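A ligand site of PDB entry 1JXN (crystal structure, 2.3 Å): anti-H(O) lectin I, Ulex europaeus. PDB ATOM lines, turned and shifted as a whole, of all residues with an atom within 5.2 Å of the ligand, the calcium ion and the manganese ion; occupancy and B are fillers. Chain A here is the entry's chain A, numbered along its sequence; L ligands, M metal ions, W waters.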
ATOM      1  N   GLU A  44       3.275  -9.579   3.374  1.00  0.00           N
ATOM      2  CA  GLU A  44       3.344 -10.777   2.516  1.00  0.00           C
ATOM      3  C   GLU A  44       4.123 -10.400   1.254  1.00  0.00           C
ATOM      4  O   GLU A  44       3.560  -9.783   0.344  1.00  0.00           O
ATOM      5  CB  GLU A  44       1.934 -11.225   2.124  1.00  0.00           C
ATOM      6  CG  GLU A  44       1.073 -11.676   3.281  1.00  0.00           C
ATOM      7  CD  GLU A  44      -0.383 -11.748   2.917  1.00  0.00           C
ATOM      8  OE1 GLU A  44      -0.849 -10.852   2.185  1.00  0.00           O
ATOM      9  OE2 GLU A  44      -1.063 -12.692   3.359  1.00  0.00           O
ATOM     10  N   THR A  86       8.690 -18.835   7.249  1.00  0.00           N
ATOM     11  CA  THR A  86       7.716 -18.958   6.162  1.00  0.00           C
ATOM     12  C   THR A  86       8.375 -18.505   4.829  1.00  0.00           C
ATOM     13  O   THR A  86       9.438 -17.865   4.856  1.00  0.00           O
ATOM     14  CB  THR A  86       6.526 -17.997   6.428  1.00  0.00           C
ATOM     15  OG1 THR A  86       6.933 -16.621   6.311  1.00  0.00           O
ATOM     16  CG2 THR A  86       5.978 -18.239   7.805  1.00  0.00           C
ATOM     17  N   ASP A  87       7.839 -18.893   3.666  1.00  0.00           N
ATOM     18  CA  ASP A  87       6.643 -19.724   3.449  1.00  0.00           C
ATOM     19  C   ASP A  87       7.075 -20.795   2.471  1.00  0.00           C
ATOM     20  O   ASP A  87       6.409 -21.821   2.340  1.00  0.00           O
ATOM     21  CB  ASP A  87       5.559 -18.932   2.773  1.00  0.00           C
ATOM     22  CG  ASP A  87       4.743 -18.148   3.731  1.00  0.00           C
ATOM     23  OD1 ASP A  87       5.058 -16.957   3.948  1.00  0.00           O
ATOM     24  OD2 ASP A  87       3.772 -18.721   4.282  1.00  0.00           O
ATOM     25  N   ARG A 102      -1.084 -12.927  -4.585  1.00  0.00           N
ATOM     26  CA  ARG A 102      -0.810 -12.839  -3.154  1.00  0.00           C
ATOM     27  C   ARG A 102       0.380 -13.673  -2.762  1.00  0.00           C
ATOM     28  O   ARG A 102       0.476 -14.842  -3.155  1.00  0.00           O
ATOM     29  CB  ARG A 102      -2.032 -13.254  -2.355  1.00  0.00           C
ATOM     30  CG  ARG A 102      -1.870 -13.042  -0.871  1.00  0.00           C
ATOM     31  CD  ARG A 102      -3.186 -13.150  -0.191  1.00  0.00           C
ATOM     32  NE  ARG A 102      -3.043 -13.246   1.251  1.00  0.00           N
ATOM     33  CZ  ARG A 102      -4.011 -13.665   2.060  1.00  0.00           C
ATOM     34  NH1 ARG A 102      -5.192 -14.002   1.545  1.00  0.00           N
ATOM     35  NH2 ARG A 102      -3.797 -13.764   3.362  1.00  0.00           N
ATOM     36  N   ALA A 103       1.265 -13.079  -1.971  1.00  0.00           N
ATOM     37  CA  ALA A 103       2.469 -13.744  -1.515  1.00  0.00           C
ATOM     38  C   ALA A 103       2.255 -14.379  -0.154  1.00  0.00           C
ATOM     39  O   ALA A 103       1.119 -14.581   0.270  1.00  0.00           O
ATOM     40  CB  ALA A 103       3.619 -12.748  -1.468  1.00  0.00           C
ATOM     41  N   GLY A 104       3.341 -14.690   0.548  1.00  0.00           N
ATOM     42  CA  GLY A 104       3.187 -15.323   1.842  1.00  0.00           C
ATOM     43  C   GLY A 104       2.860 -16.787   1.620  1.00  0.00           C
ATOM     44  O   GLY A 104       3.564 -17.473   0.870  1.00  0.00           O
ATOM     45  N   GLY A 105       1.792 -17.255   2.249  1.00  0.00           N
ATOM     46  CA  GLY A 105       1.409 -18.648   2.111  1.00  0.00           C
ATOM     47  C   GLY A 105       0.839 -19.006   0.761  1.00  0.00           C
ATOM     48  O   GLY A 105       0.688 -20.180   0.434  1.00  0.00           O
ATOM     49  N   TYR A 106       0.513 -17.996  -0.029  1.00  0.00           N
ATOM     50  CA  TYR A 106      -0.061 -18.217  -1.342  1.00  0.00           C
ATOM     51  C   TYR A 106       0.975 -18.277  -2.446  1.00  0.00           C
ATOM     52  O   TYR A 106       0.636 -18.524  -3.603  1.00  0.00           O
ATOM     53  CB  TYR A 106      -1.123 -17.172  -1.614  1.00  0.00           C
ATOM     54  CG  TYR A 106      -2.269 -17.287  -0.638  1.00  0.00           C
ATOM     55  CD1 TYR A 106      -2.256 -16.576   0.581  1.00  0.00           C
ATOM     56  CD2 TYR A 106      -3.363 -18.114  -0.906  1.00  0.00           C
ATOM     57  CE1 TYR A 106      -3.308 -16.702   1.491  1.00  0.00           C
ATOM     58  CE2 TYR A 106      -4.405 -18.245  -0.005  1.00  0.00           C
ATOM     59  CZ  TYR A 106      -4.372 -17.528   1.190  1.00  0.00           C
ATOM     60  OH  TYR A 106      -5.434 -17.627   2.031  1.00  0.00           O
ATOM     61  N   PHE A 107       2.240 -18.052  -2.086  1.00  0.00           N
ATOM     62  CA  PHE A 107       3.381 -18.120  -2.999  1.00  0.00           C
ATOM     63  C   PHE A 107       3.449 -17.182  -4.213  1.00  0.00           C
ATOM     64  O   PHE A 107       4.415 -17.232  -4.976  1.00  0.00           O
ATOM     65  CB  PHE A 107       3.537 -19.559  -3.496  1.00  0.00           C
ATOM     66  CG  PHE A 107       3.753 -20.557  -2.402  1.00  0.00           C
ATOM     67  CD1 PHE A 107       2.758 -21.474  -2.074  1.00  0.00           C
ATOM     68  CD2 PHE A 107       4.972 -20.597  -1.713  1.00  0.00           C
ATOM     69  CE1 PHE A 107       2.960 -22.417  -1.075  1.00  0.00           C
ATOM     70  CE2 PHE A 107       5.188 -21.533  -0.701  1.00  0.00           C
ATOM     71  CZ  PHE A 107       4.187 -22.441  -0.372  1.00  0.00           C
ATOM     72  N   GLU A 125       5.012 -27.342  -4.867  1.00  0.00           N
ATOM     73  CA  GLU A 125       5.431 -26.514  -3.762  1.00  0.00           C
ATOM     74  C   GLU A 125       6.327 -27.196  -2.735  1.00  0.00           C
ATOM     75  O   GLU A 125       6.346 -28.413  -2.604  1.00  0.00           O
ATOM     76  CB  GLU A 125       4.218 -25.919  -3.038  1.00  0.00           C
ATOM     77  CG  GLU A 125       3.316 -26.957  -2.395  1.00  0.00           C
ATOM     78  CD  GLU A 125       2.433 -26.393  -1.316  1.00  0.00           C
ATOM     79  OE1 GLU A 125       2.559 -26.843  -0.163  1.00  0.00           O
ATOM     80  OE2 GLU A 125       1.599 -25.509  -1.604  1.00  0.00           O
ATOM     81  N   ASP A 127       6.573 -26.123   0.775  1.00  0.00           N
ATOM     82  CA  ASP A 127       5.958 -25.316   1.818  1.00  0.00           C
ATOM     83  C   ASP A 127       6.670 -25.444   3.162  1.00  0.00           C
ATOM     84  O   ASP A 127       6.732 -26.533   3.731  1.00  0.00           O
ATOM     85  CB  ASP A 127       4.498 -25.760   1.958  1.00  0.00           C
ATOM     86  CG  ASP A 127       3.636 -24.743   2.628  1.00  0.00           C
ATOM     87  OD1 ASP A 127       2.442 -24.668   2.274  1.00  0.00           O
ATOM     88  OD2 ASP A 127       4.126 -23.999   3.495  1.00  0.00           O
ATOM     89  N   ILE A 129       5.828 -23.614   6.052  1.00  0.00           N
ATOM     90  CA  ILE A 129       4.966 -23.367   7.226  1.00  0.00           C
ATOM     91  C   ILE A 129       3.493 -23.759   6.983  1.00  0.00           C
ATOM     92  O   ILE A 129       2.793 -23.182   6.134  1.00  0.00           O
ATOM     93  CB  ILE A 129       5.078 -21.912   7.753  1.00  0.00           C
ATOM     94  CG1 ILE A 129       4.777 -21.876   9.257  1.00  0.00           C
ATOM     95  CG2 ILE A 129       4.140 -20.966   7.019  1.00  0.00           C
ATOM     96  CD1 ILE A 129       5.832 -22.527  10.139  1.00  0.00           C
ATOM     97  N   GLY A 130       3.045 -24.777   7.721  1.00  0.00           N
ATOM     98  CA  GLY A 130       1.685 -25.267   7.570  1.00  0.00           C
ATOM     99  C   GLY A 130       0.787 -24.895   8.727  1.00  0.00           C
ATOM    100  O   GLY A 130       1.027 -23.890   9.418  1.00  0.00           O
ATOM    101  N   VAL A 133      -0.752 -22.183  11.530  1.00  0.00           N
ATOM    102  CA  VAL A 133      -0.418 -20.849  10.992  1.00  0.00           C
ATOM    103  C   VAL A 133      -1.066 -20.684   9.604  1.00  0.00           C
ATOM    104  O   VAL A 133      -1.699 -19.654   9.314  1.00  0.00           O
ATOM    105  CB  VAL A 133       1.112 -20.672  10.848  1.00  0.00           C
ATOM    106  CG1 VAL A 133       1.423 -19.255  10.382  1.00  0.00           C
ATOM    107  CG2 VAL A 133       1.805 -20.991  12.177  1.00  0.00           C
ATOM    108  N   ASN A 134      -0.893 -21.705   8.754  1.00  0.00           N
ATOM    109  CA  ASN A 134      -1.473 -21.757   7.416  1.00  0.00           C
ATOM    110  C   ASN A 134      -2.550 -22.823   7.504  1.00  0.00           C
ATOM    111  O   ASN A 134      -2.304 -24.005   7.287  1.00  0.00           O
ATOM    112  CB  ASN A 134      -0.417 -22.164   6.376  1.00  0.00           C
ATOM    113  CG  ASN A 134       0.291 -20.966   5.743  1.00  0.00           C
ATOM    114  OD1 ASN A 134       1.103 -21.131   4.833  1.00  0.00           O
ATOM    115  ND2 ASN A 134      -0.018 -19.758   6.222  1.00  0.00           N
ATOM    116  N   TRP A 136      -5.138 -24.071   5.777  1.00  0.00           N
ATOM    117  CA  TRP A 136      -5.322 -25.007   4.651  1.00  0.00           C
ATOM    118  C   TRP A 136      -4.262 -26.085   4.433  1.00  0.00           C
ATOM    119  O   TRP A 136      -4.414 -26.927   3.537  1.00  0.00           O
ATOM    120  CB  TRP A 136      -5.425 -24.215   3.341  1.00  0.00           C
ATOM    121  CG  TRP A 136      -4.209 -23.369   3.082  1.00  0.00           C
ATOM    122  CD1 TRP A 136      -3.073 -23.743   2.397  1.00  0.00           C
ATOM    123  CD2 TRP A 136      -3.980 -22.027   3.514  1.00  0.00           C
ATOM    124  NE1 TRP A 136      -2.173 -22.708   2.377  1.00  0.00           N
ATOM    125  CE2 TRP A 136      -2.701 -21.639   3.048  1.00  0.00           C
ATOM    126  CE3 TRP A 136      -4.747 -21.102   4.243  1.00  0.00           C
ATOM    127  CZ2 TRP A 136      -2.175 -20.373   3.293  1.00  0.00           C
ATOM    128  CZ3 TRP A 136      -4.211 -19.840   4.479  1.00  0.00           C
ATOM    129  CH2 TRP A 136      -2.934 -19.488   4.005  1.00  0.00           C
ATOM    130  N   ASP A 137      -3.191 -26.031   5.215  1.00  0.00           N
ATOM    131  CA  ASP A 137      -2.076 -26.981   5.104  1.00  0.00           C
ATOM    132  C   ASP A 137      -1.990 -27.996   6.225  1.00  0.00           C
ATOM    133  O   ASP A 137      -2.551 -27.790   7.313  1.00  0.00           O
ATOM    134  CB  ASP A 137      -0.741 -26.247   5.208  1.00  0.00           C
ATOM    135  CG  ASP A 137      -0.397 -25.463   3.986  1.00  0.00           C
ATOM    136  OD1 ASP A 137       0.260 -24.415   4.162  1.00  0.00           O
ATOM    137  OD2 ASP A 137      -0.734 -25.897   2.868  1.00  0.00           O
ATOM    138  N   PRO A 138      -1.253 -29.093   5.993  1.00  0.00           N
ATOM    139  CA  PRO A 138      -1.083 -30.110   7.022  1.00  0.00           C
ATOM    140  C   PRO A 138      -0.288 -29.462   8.166  1.00  0.00           C
ATOM    141  O   PRO A 138       0.222 -28.341   8.032  1.00  0.00           O
ATOM    142  CB  PRO A 138      -0.265 -31.210   6.304  1.00  0.00           C
ATOM    143  CG  PRO A 138       0.296 -30.539   5.099  1.00  0.00           C
ATOM    144  CD  PRO A 138      -0.808 -29.621   4.691  1.00  0.00           C
ATOM    145  N   HIS A 142       6.172 -29.109   4.445  1.00  0.00           N
ATOM    146  CA  HIS A 142       6.012 -30.202   3.493  1.00  0.00           C
ATOM    147  C   HIS A 142       6.200 -29.786   2.032  1.00  0.00           C
ATOM    148  O   HIS A 142       6.472 -28.613   1.716  1.00  0.00           O
ATOM    149  CB  HIS A 142       4.592 -30.766   3.642  1.00  0.00           C
ATOM    150  CG  HIS A 142       3.531 -29.765   3.346  1.00  0.00           C
ATOM    151  ND1 HIS A 142       3.372 -28.589   4.044  1.00  0.00           N
ATOM    152  CD2 HIS A 142       2.631 -29.718   2.335  1.00  0.00           C
ATOM    153  CE1 HIS A 142       2.427 -27.862   3.443  1.00  0.00           C
ATOM    154  NE2 HIS A 142       1.941 -28.504   2.401  1.00  0.00           N
ATOM    155  N   VAL A 150      -4.233 -23.332  -3.692  1.00  0.00           N
ATOM    156  CA  VAL A 150      -3.138 -23.268  -2.720  1.00  0.00           C
ATOM    157  C   VAL A 150      -3.100 -24.501  -1.804  1.00  0.00           C
ATOM    158  O   VAL A 150      -2.107 -24.739  -1.105  1.00  0.00           O
ATOM    159  CB  VAL A 150      -3.214 -22.005  -1.844  1.00  0.00           C
ATOM    160  CG1 VAL A 150      -4.365 -22.100  -0.859  1.00  0.00           C
ATOM    161  CG2 VAL A 150      -1.893 -21.782  -1.164  1.00  0.00           C
ATOM    162  N   SER A 152      -2.943 -28.420  -1.605  1.00  0.00           N
ATOM    163  CA  SER A 152      -2.463 -29.534  -2.421  1.00  0.00           C
ATOM    164  C   SER A 152      -3.438 -30.696  -2.676  1.00  0.00           C
ATOM    165  O   SER A 152      -4.431 -30.876  -1.943  1.00  0.00           O
ATOM    166  CB  SER A 152      -1.186 -30.103  -1.813  1.00  0.00           C
ATOM    167  OG  SER A 152      -0.231 -29.094  -1.592  1.00  0.00           O
ATOM    168  N   TYR A 219       7.152 -14.078   5.225  1.00  0.00           N
ATOM    169  CA  TYR A 219       6.204 -13.219   5.922  1.00  0.00           C
ATOM    170  C   TYR A 219       6.872 -12.381   7.017  1.00  0.00           C
ATOM    171  O   TYR A 219       7.821 -12.832   7.647  1.00  0.00           O
ATOM    172  CB  TYR A 219       5.114 -14.099   6.539  1.00  0.00           C
ATOM    173  CG  TYR A 219       4.003 -13.364   7.261  1.00  0.00           C
ATOM    174  CD1 TYR A 219       3.774 -13.573   8.619  1.00  0.00           C
ATOM    175  CD2 TYR A 219       3.141 -12.508   6.575  1.00  0.00           C
ATOM    176  CE1 TYR A 219       2.721 -12.959   9.282  1.00  0.00           C
ATOM    177  CE2 TYR A 219       2.095 -11.885   7.209  1.00  0.00           C
ATOM    178  CZ  TYR A 219       1.883 -12.118   8.563  1.00  0.00           C
ATOM    179  OH  TYR A 219       0.790 -11.539   9.195  1.00  0.00           O
ATOM    180  N   ARG A 222       8.552 -13.733  10.286  1.00  0.00           N
ATOM    181  CA  ARG A 222       9.085 -15.061   9.980  1.00  0.00           C
ATOM    182  C   ARG A 222       9.806 -15.033   8.615  1.00  0.00           C
ATOM    183  O   ARG A 222       9.681 -15.984   7.830  1.00  0.00           O
ATOM    184  CB  ARG A 222       7.944 -16.091   9.959  1.00  0.00           C
ATOM    185  CG  ARG A 222       7.077 -16.089  11.212  1.00  0.00           C
ATOM    186  CD  ARG A 222       5.753 -16.822  10.985  1.00  0.00           C
ATOM    187  NE  ARG A 222       5.716 -18.151  11.592  1.00  0.00           N
ATOM    188  CZ  ARG A 222       4.836 -18.541  12.511  1.00  0.00           C
ATOM    189  NH1 ARG A 222       3.912 -17.687  12.960  1.00  0.00           N
ATOM    190  NH2 ARG A 222       4.875 -19.764  12.990  1.00  0.00           N
HETATM  191  C1  LIG L   1      -0.865 -16.158   7.217  1.00  0.00           C
HETATM  192  C2  LIG L   1      -1.008 -16.129   5.671  1.00  0.00           C
HETATM  193  C3  LIG L   1       0.256 -15.433   5.110  1.00  0.00           C
HETATM  194  C4  LIG L   1       1.515 -16.219   5.559  1.00  0.00           C
HETATM  195  C5  LIG L   1       1.579 -16.260   7.088  1.00  0.00           C
HETATM  196  C6  LIG L   1       2.823 -17.046   7.553  1.00  0.00           C
HETATM  197  O1  LIG L   1      -0.857 -14.768   7.721  1.00  0.00           O
HETATM  198  O2  LIG L   1      -2.210 -15.451   5.301  1.00  0.00           O
HETATM  199  O3  LIG L   1       0.181 -15.381   3.699  1.00  0.00           O
HETATM  200  O4  LIG L   1       1.455 -17.557   5.051  1.00  0.00           O
HETATM  201  O5  LIG L   1       0.376 -16.850   7.616  1.00  0.00           O
HETATM  202  C7  LIG L   1      -1.887 -13.752   7.844  1.00  0.00           C
HETATM  203 CA    CA M   1       2.005 -23.024   3.743  1.00  0.00          CA
HETATM  204 MN    MN M   2       1.030 -26.174   1.294  1.00  0.00          MN
HETATM  205  O   HOH W   1       0.609 -22.304   1.987  1.00  0.00           O
HETATM  206  O   HOH W   2      -0.157 -24.516   0.445  1.00  0.00           O
HETATM  207  O   HOH W   3       3.372 -21.310   3.300  1.00  0.00           O
HETATM  208  O   HOH W   4       0.055 -28.017   0.680  1.00  0.00           O
HETATM  209  O   HOH W   5      -3.904 -16.089   8.369  1.00  0.00           O
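The side-chain carboxylate of Asp 87 is in hydrogen-bond range of an oxygen (O4) of the ligand. NH2 of Arg 102 is in hydrogen-bond range of O2 of the ligand, at 3.0 Å. ND2 of Asn 134 lies within hydrogen-bond range of O4 of the ligand, at 2.9 Å. An oxygen (O4) of the ligand is in hydrogen-bond range of the backbone NH (N) of Gly 105. The side-chain carboxylate of Glu 44 lies within hydrogen-bond range of an oxygen (O3) of the ligand (3.0 Å).
The side-chain hydroxyl (OG1) of Thr 86 lies within hydrogen-bond range of the backbone NH (N) of Tyr 219 (2.8 Å). N of Thr 86 lies within hydrogen-bond range of O of Arg 222 (3.1 Å). OE2 of Glu 44 is in salt-bridge range of NH2 of Arg 102, 2.9 Å away. The side-chain carboxylate of Asp 87 sits at hydrogen-bond distance from the side-chain hydroxyl of Thr 86, 3.0 Å away. N of Asp 127 is in hydrogen-bond range of O of His 142 (2.7 Å). A ring nitrogen (NE2) of His 142 sits close to the side-chain carboxylate of Glu 125 (3.1 Å). OD1 of Asp 137 sits close to NE1 of Trp 136 (3.5 Å). OD2 of Asp 87 is in hydrogen-bond range of N of Gly 105 (3.2 Å).
Residues that only touch the ligand: Thr 86, Ala 103, Gly 104, Val 133 and Tyr 219. Hydrophobic or aromatic side chains that line the ligand: Val 133 and Tyr 219. Of the 23 residues printed, 10 come within 4 Å of the ligand.
Of the 23 residues printed, 4 come within 4 Å of the calcium ion. The nearest printed residue that does not touch the calcium ion is Trp 136 (4.4 Å).
Within 4 Å of the manganese ion: Glu 125, Asp 127, Asp 137 and His 142. The nearest printed residue that does not touch the manganese ion is Val 150 (4.2 Å).
The calcium ion is bound by water W3 (2.2 Å), the side-chain carboxylate (OD1) of Asp 127 (2.2 Å), the side-chain carboxylate (OD1) of Asp 137 (2.3 Å), the side-chain carboxylate (OD2) of Asp 127 (2.3 Å), water W1 (2.4 Å), the side-chain amide oxygen (OD1) of Asn 134 (2.4 Å) and the backbone carbonyl oxygen (O) of Ile 129 (2.5 Å). The calcium ion has seven donor atoms within binding distance.
Water W4 binds the manganese ion. Water W2 binds the manganese ion (2.2 Å). The side-chain carboxylate (OE1) of Glu 125 is bound to the manganese ion (2.2 Å). The manganese ion is bound by OD1 of Asp 127 (2.3 Å). The manganese ion is bound by OD2 of Asp 137, 2.4 Å away. Slightly farther from the manganese ion lies NE2 of His 142 (2.7 Å).
Water W1 bridges O of Gly 105 (2.6 Å) and NE1 of Trp 136 (2.8 Å). Water W4 bridges the side-chain hydroxyl (OG) of Ser 152 and a ring nitrogen (NE2) of His 142. Water W2 lies within hydrogen-bond range of the backbone carbonyl oxygen of Val 150 (2.5 Å), the side-chain carboxylate of Glu 125 (2.9 Å) and the indole nitrogen of Trp 136 (3.3 Å).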
